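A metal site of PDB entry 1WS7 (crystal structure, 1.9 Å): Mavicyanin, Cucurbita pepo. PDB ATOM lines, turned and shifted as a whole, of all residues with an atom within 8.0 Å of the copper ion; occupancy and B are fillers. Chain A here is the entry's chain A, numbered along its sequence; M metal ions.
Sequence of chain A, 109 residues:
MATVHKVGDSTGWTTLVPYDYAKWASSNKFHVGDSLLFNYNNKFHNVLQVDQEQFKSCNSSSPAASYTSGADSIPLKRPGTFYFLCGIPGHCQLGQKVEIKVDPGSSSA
Thr 15 touches the copper ion.
Phe 44 touches the copper ion.
CG1 of Ile 88 touches the copper ion, 3.97 Å away.
Seven residues have an atom within 4 Å of the copper ion: Thr 15, Phe 44, His 45, Cys 86, Ile 88, His 91 and Gln 96.
The nearest printed residue that does not touch the copper ion is Asn 46 (4.7 Å).
The side-chain hydroxyl (OG1) of Thr 15 lies close to a ring nitrogen (ND1) of His 45.
The side-chain hydroxyl of Thr 15 sits close to a ring nitrogen (ND1) of His 91 (3.5 Å).
SG of Cys 86 sits close to N of Ile 88 (3.5 Å).
The backbone NH (N) of Asn 46 sits close to the side-chain sulfur (SG) of Cys 86, at 3.6 Å.
The side-chain hydroxyl (OG1) of Thr 15 sits close to the side-chain amide oxygen (OE1) of Gln 96, 2.6 Å away.
The side-chain amide nitrogen (NE2) of Gln 96 sits close to the indole nitrogen (NE1) of Trp 13 (3.4 Å).
The copper ion is bound by ND1 of His 45 (2.0 Å), ND1 of His 91 (2.1 Å), SG of Cys 86 (2.2 Å) and OE1 of Gln 96 (2.6 Å).
The copper ion has four donor atoms within binding distance.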
ATOM      1  N   TRP A  13      10.059  25.446  26.980  1.00  0.00           N
ATOM      2  CA  TRP A  13       9.140  24.308  27.102  1.00  0.00           C
ATOM      3  C   TRP A  13      10.021  23.094  27.399  1.00  0.00           C
ATOM      4  O   TRP A  13      10.767  22.636  26.547  1.00  0.00           O
ATOM      5  CB  TRP A  13       8.414  24.143  25.749  1.00  0.00           C
ATOM      6  CG  TRP A  13       7.296  23.141  25.684  1.00  0.00           C
ATOM      7  CD1 TRP A  13       7.211  22.085  24.812  1.00  0.00           C
ATOM      8  CD2 TRP A  13       6.056  23.173  26.406  1.00  0.00           C
ATOM      9  NE1 TRP A  13       5.986  21.473  24.947  1.00  0.00           N
ATOM     10  CE2 TRP A  13       5.262  22.105  25.915  1.00  0.00           C
ATOM     11  CE3 TRP A  13       5.537  23.993  27.419  1.00  0.00           C
ATOM     12  CZ2 TRP A  13       3.971  21.849  26.398  1.00  0.00           C
ATOM     13  CZ3 TRP A  13       4.256  23.728  27.905  1.00  0.00           C
ATOM     14  CH2 TRP A  13       3.492  22.667  27.393  1.00  0.00           C
ATOM     15  N   THR A  14       9.923  22.575  28.623  1.00  0.00           N
ATOM     16  CA  THR A  14      10.774  21.459  29.036  1.00  0.00           C
ATOM     17  C   THR A  14      10.161  20.640  30.173  1.00  0.00           C
ATOM     18  O   THR A  14       9.173  21.035  30.783  1.00  0.00           O
ATOM     19  CB  THR A  14      12.144  22.007  29.534  1.00  0.00           C
ATOM     20  OG1 THR A  14      13.023  20.920  29.866  1.00  0.00           O
ATOM     21  CG2 THR A  14      11.949  22.863  30.781  1.00  0.00           C
ATOM     22  N   THR A  15      10.777  19.484  30.451  1.00  0.00           N
ATOM     23  CA  THR A  15      10.340  18.611  31.539  1.00  0.00           C
ATOM     24  C   THR A  15      11.547  18.394  32.454  1.00  0.00           C
ATOM     25  O   THR A  15      11.445  17.729  33.482  1.00  0.00           O
ATOM     26  CB  THR A  15       9.886  17.209  31.030  1.00  0.00           C
ATOM     27  OG1 THR A  15       9.462  17.286  29.668  1.00  0.00           O
ATOM     28  CG2 THR A  15       8.730  16.708  31.877  1.00  0.00           C
ATOM     29  N   LEU A  16      12.689  18.976  32.074  1.00  0.00           N
ATOM     30  CA  LEU A  16      13.934  18.816  32.827  1.00  0.00           C
ATOM     31  C   LEU A  16      13.744  18.966  34.333  1.00  0.00           C
ATOM     32  O   LEU A  16      14.193  18.134  35.122  1.00  0.00           O
ATOM     33  CB  LEU A  16      14.982  19.814  32.324  1.00  0.00           C
ATOM     34  CG  LEU A  16      16.460  19.402  32.442  1.00  0.00           C
ATOM     35  CD1 LEU A  16      16.813  19.091  33.883  1.00  0.00           C
ATOM     36  CD2 LEU A  16      16.720  18.188  31.550  1.00  0.00           C
ATOM     37  N   TYR A  40      11.961  24.553  22.416  1.00  0.00           N
ATOM     38  CA  TYR A  40      12.322  23.258  22.988  1.00  0.00           C
ATOM     39  C   TYR A  40      13.123  22.417  22.004  1.00  0.00           C
ATOM     40  O   TYR A  40      13.225  22.761  20.824  1.00  0.00           O
ATOM     41  CB  TYR A  40      11.036  22.493  23.356  1.00  0.00           C
ATOM     42  CG  TYR A  40      10.111  22.279  22.166  1.00  0.00           C
ATOM     43  CD1 TYR A  40      10.164  21.103  21.411  1.00  0.00           C
ATOM     44  CD2 TYR A  40       9.191  23.263  21.781  1.00  0.00           C
ATOM     45  CE1 TYR A  40       9.336  20.921  20.299  1.00  0.00           C
ATOM     46  CE2 TYR A  40       8.352  23.080  20.670  1.00  0.00           C
ATOM     47  CZ  TYR A  40       8.435  21.903  19.937  1.00  0.00           C
ATOM     48  OH  TYR A  40       7.617  21.719  18.847  1.00  0.00           O
ATOM     49  N   ASN A  41      13.689  21.334  22.499  1.00  0.00           N
ATOM     50  CA  ASN A  41      14.454  20.417  21.652  1.00  0.00           C
ATOM     51  C   ASN A  41      13.377  19.519  21.034  1.00  0.00           C
ATOM     52  O   ASN A  41      12.803  18.687  21.747  1.00  0.00           O
ATOM     53  CB  ASN A  41      15.394  19.575  22.518  1.00  0.00           C
ATOM     54  CG  ASN A  41      16.186  18.574  21.699  1.00  0.00           C
ATOM     55  OD1 ASN A  41      15.821  18.255  20.567  1.00  0.00           O
ATOM     56  ND2 ASN A  41      17.264  18.054  22.283  1.00  0.00           N
ATOM     57  N   LYS A  43      13.451  16.952  19.555  1.00  0.00           N
ATOM     58  CA  LYS A  43      13.792  15.541  19.523  1.00  0.00           C
ATOM     59  C   LYS A  43      13.269  14.939  20.828  1.00  0.00           C
ATOM     60  O   LYS A  43      13.189  13.726  20.967  1.00  0.00           O
ATOM     61  CB  LYS A  43      15.306  15.348  19.429  1.00  0.00           C
ATOM     62  CG  LYS A  43      15.900  15.722  18.083  1.00  0.00           C
ATOM     63  CD  LYS A  43      15.222  14.944  16.973  1.00  0.00           C
ATOM     64  CE  LYS A  43      15.744  15.347  15.605  1.00  0.00           C
ATOM     65  NZ  LYS A  43      14.955  14.702  14.512  1.00  0.00           N
ATOM     66  N   PHE A  44      12.877  15.807  21.758  1.00  0.00           N
ATOM     67  CA  PHE A  44      12.360  15.371  23.053  1.00  0.00           C
ATOM     68  C   PHE A  44      10.895  15.666  23.296  1.00  0.00           C
ATOM     69  O   PHE A  44      10.198  14.886  23.936  1.00  0.00           O
ATOM     70  CB  PHE A  44      13.159  16.010  24.190  1.00  0.00           C
ATOM     71  CG  PHE A  44      14.391  15.247  24.594  1.00  0.00           C
ATOM     72  CD1 PHE A  44      15.534  15.303  23.810  1.00  0.00           C
ATOM     73  CD2 PHE A  44      14.388  14.467  25.735  1.00  0.00           C
ATOM     74  CE1 PHE A  44      16.673  14.584  24.175  1.00  0.00           C
ATOM     75  CE2 PHE A  44      15.527  13.741  26.113  1.00  0.00           C
ATOM     76  CZ  PHE A  44      16.659  13.806  25.325  1.00  0.00           C
ATOM     77  N   HIS A  45      10.425  16.808  22.798  1.00  0.00           N
ATOM     78  CA  HIS A  45       9.040  17.234  23.036  1.00  0.00           C
ATOM     79  C   HIS A  45       8.292  17.665  21.781  1.00  0.00           C
ATOM     80  O   HIS A  45       8.847  17.738  20.693  1.00  0.00           O
ATOM     81  CB  HIS A  45       9.033  18.416  24.001  1.00  0.00           C
ATOM     82  CG  HIS A  45       9.988  18.281  25.142  1.00  0.00           C
ATOM     83  ND1 HIS A  45       9.750  17.439  26.208  1.00  0.00           N
ATOM     84  CD2 HIS A  45      11.188  18.871  25.380  1.00  0.00           C
ATOM     85  CE1 HIS A  45      10.763  17.511  27.058  1.00  0.00           C
ATOM     86  NE2 HIS A  45      11.651  18.378  26.578  1.00  0.00           N
ATOM     87  N   ASN A  46       7.009  17.952  21.982  1.00  0.00           N
ATOM     88  CA  ASN A  46       6.150  18.481  20.933  1.00  0.00           C
ATOM     89  C   ASN A  46       5.129  19.360  21.623  1.00  0.00           C
ATOM     90  O   ASN A  46       5.139  19.463  22.859  1.00  0.00           O
ATOM     91  CB  ASN A  46       5.487  17.352  20.111  1.00  0.00           C
ATOM     92  CG  ASN A  46       4.502  16.493  20.909  1.00  0.00           C
ATOM     93  OD1 ASN A  46       4.183  15.382  20.493  1.00  0.00           O
ATOM     94  ND2 ASN A  46       4.008  17.009  22.016  1.00  0.00           N
ATOM     95  N   VAL A  47       4.274  20.017  20.849  1.00  0.00           N
ATOM     96  CA  VAL A  47       3.247  20.877  21.409  1.00  0.00           C
ATOM     97  C   VAL A  47       1.917  20.471  20.785  1.00  0.00           C
ATOM     98  O   VAL A  47       1.740  20.570  19.563  1.00  0.00           O
ATOM     99  CB  VAL A  47       3.518  22.363  21.088  1.00  0.00           C
ATOM    100  CG1 VAL A  47       2.449  23.233  21.726  1.00  0.00           C
ATOM    101  CG2 VAL A  47       4.900  22.769  21.599  1.00  0.00           C
ATOM    102  N   LEU A  85      -0.228  20.858  25.641  1.00  0.00           N
ATOM    103  CA  LEU A  85       0.541  19.917  26.436  1.00  0.00           C
ATOM    104  C   LEU A  85       1.524  19.162  25.549  1.00  0.00           C
ATOM    105  O   LEU A  85       1.357  19.134  24.324  1.00  0.00           O
ATOM    106  CB  LEU A  85      -0.390  18.921  27.152  1.00  0.00           C
ATOM    107  CG  LEU A  85      -1.390  18.097  26.315  1.00  0.00           C
ATOM    108  CD1 LEU A  85      -0.672  17.022  25.515  1.00  0.00           C
ATOM    109  CD2 LEU A  85      -2.405  17.448  27.256  1.00  0.00           C
ATOM    110  N   CYS A  86       2.546  18.595  26.166  1.00  0.00           N
ATOM    111  CA  CYS A  86       3.499  17.803  25.404  1.00  0.00           C
ATOM    112  C   CYS A  86       2.927  16.396  25.415  1.00  0.00           C
ATOM    113  O   CYS A  86       2.572  15.867  26.474  1.00  0.00           O
ATOM    114  CB  CYS A  86       4.884  17.791  26.055  1.00  0.00           C
ATOM    115  SG  CYS A  86       5.981  16.645  25.199  1.00  0.00           S
ATOM    116  N   GLY A  87       2.849  15.781  24.239  1.00  0.00           N
ATOM    117  CA  GLY A  87       2.281  14.455  24.142  1.00  0.00           C
ATOM    118  C   GLY A  87       3.209  13.279  24.409  1.00  0.00           C
ATOM    119  O   GLY A  87       2.743  12.146  24.465  1.00  0.00           O
ATOM    120  N   ILE A  88       4.501  13.523  24.557  1.00  0.00           N
ATOM    121  CA  ILE A  88       5.414  12.414  24.813  1.00  0.00           C
ATOM    122  C   ILE A  88       4.986  11.748  26.121  1.00  0.00           C
ATOM    123  O   ILE A  88       4.720  12.425  27.115  1.00  0.00           O
ATOM    124  CB  ILE A  88       6.877  12.893  24.897  1.00  0.00           C
ATOM    125  CG1 ILE A  88       7.194  13.780  23.684  1.00  0.00           C
ATOM    126  CG2 ILE A  88       7.813  11.694  24.888  1.00  0.00           C
ATOM    127  CD1 ILE A  88       6.840  13.149  22.355  1.00  0.00           C
ATOM    128  N   PRO A  89       4.889  10.413  26.109  1.00  0.00           N
ATOM    129  CA  PRO A  89       4.473   9.633  27.284  1.00  0.00           C
ATOM    130  C   PRO A  89       5.096  10.065  28.613  1.00  0.00           C
ATOM    131  O   PRO A  89       6.307  10.076  28.778  1.00  0.00           O
ATOM    132  CB  PRO A  89       4.862   8.210  26.902  1.00  0.00           C
ATOM    133  CG  PRO A  89       4.607   8.203  25.427  1.00  0.00           C
ATOM    134  CD  PRO A  89       5.226   9.515  24.997  1.00  0.00           C
ATOM    135  N   GLY A  90       4.225  10.435  29.550  1.00  0.00           N
ATOM    136  CA  GLY A  90       4.689  10.850  30.867  1.00  0.00           C
ATOM    137  C   GLY A  90       5.063  12.307  31.063  1.00  0.00           C
ATOM    138  O   GLY A  90       5.145  12.763  32.203  1.00  0.00           O
ATOM    139  N   HIS A  91       5.270  13.055  29.972  1.00  0.00           N
ATOM    140  CA  HIS A  91       5.660  14.453  30.113  1.00  0.00           C
ATOM    141  C   HIS A  91       4.598  15.377  30.651  1.00  0.00           C
ATOM    142  O   HIS A  91       4.864  16.198  31.531  1.00  0.00           O
ATOM    143  CB  HIS A  91       6.179  14.992  28.776  1.00  0.00           C
ATOM    144  CG  HIS A  91       7.411  14.298  28.289  1.00  0.00           C
ATOM    145  ND1 HIS A  91       8.310  14.888  27.424  1.00  0.00           N
ATOM    146  CD2 HIS A  91       7.895  13.055  28.526  1.00  0.00           C
ATOM    147  CE1 HIS A  91       9.280  14.037  27.142  1.00  0.00           C
ATOM    148  NE2 HIS A  91       9.044  12.911  27.803  1.00  0.00           N
ATOM    149  N   CYS A  92       3.383  15.262  30.120  1.00  0.00           N
ATOM    150  CA  CYS A  92       2.289  16.105  30.577  1.00  0.00           C
ATOM    151  C   CYS A  92       2.033  15.856  32.067  1.00  0.00           C
ATOM    152  O   CYS A  92       1.780  16.787  32.827  1.00  0.00           O
ATOM    153  CB  CYS A  92       1.037  15.773  29.766  1.00  0.00           C
ATOM    154  SG  CYS A  92      -0.489  16.607  30.270  1.00  0.00           S
ATOM    155  N   GLN A  96       4.256  19.340  32.096  1.00  0.00           N
ATOM    156  CA  GLN A  96       4.431  20.026  30.813  1.00  0.00           C
ATOM    157  C   GLN A  96       3.109  20.249  30.080  1.00  0.00           C
ATOM    158  O   GLN A  96       2.784  19.555  29.117  1.00  0.00           O
ATOM    159  CB  GLN A  96       5.425  19.246  29.945  1.00  0.00           C
ATOM    160  CG  GLN A  96       6.107  20.076  28.860  1.00  0.00           C
ATOM    161  CD  GLN A  96       7.199  19.301  28.152  1.00  0.00           C
ATOM    162  OE1 GLN A  96       7.376  18.108  28.391  1.00  0.00           O
ATOM    163  NE2 GLN A  96       7.929  19.979  27.273  1.00  0.00           N
HETATM  164 CU    CU M   1       7.880  16.615  26.370  1.00  0.00          CU
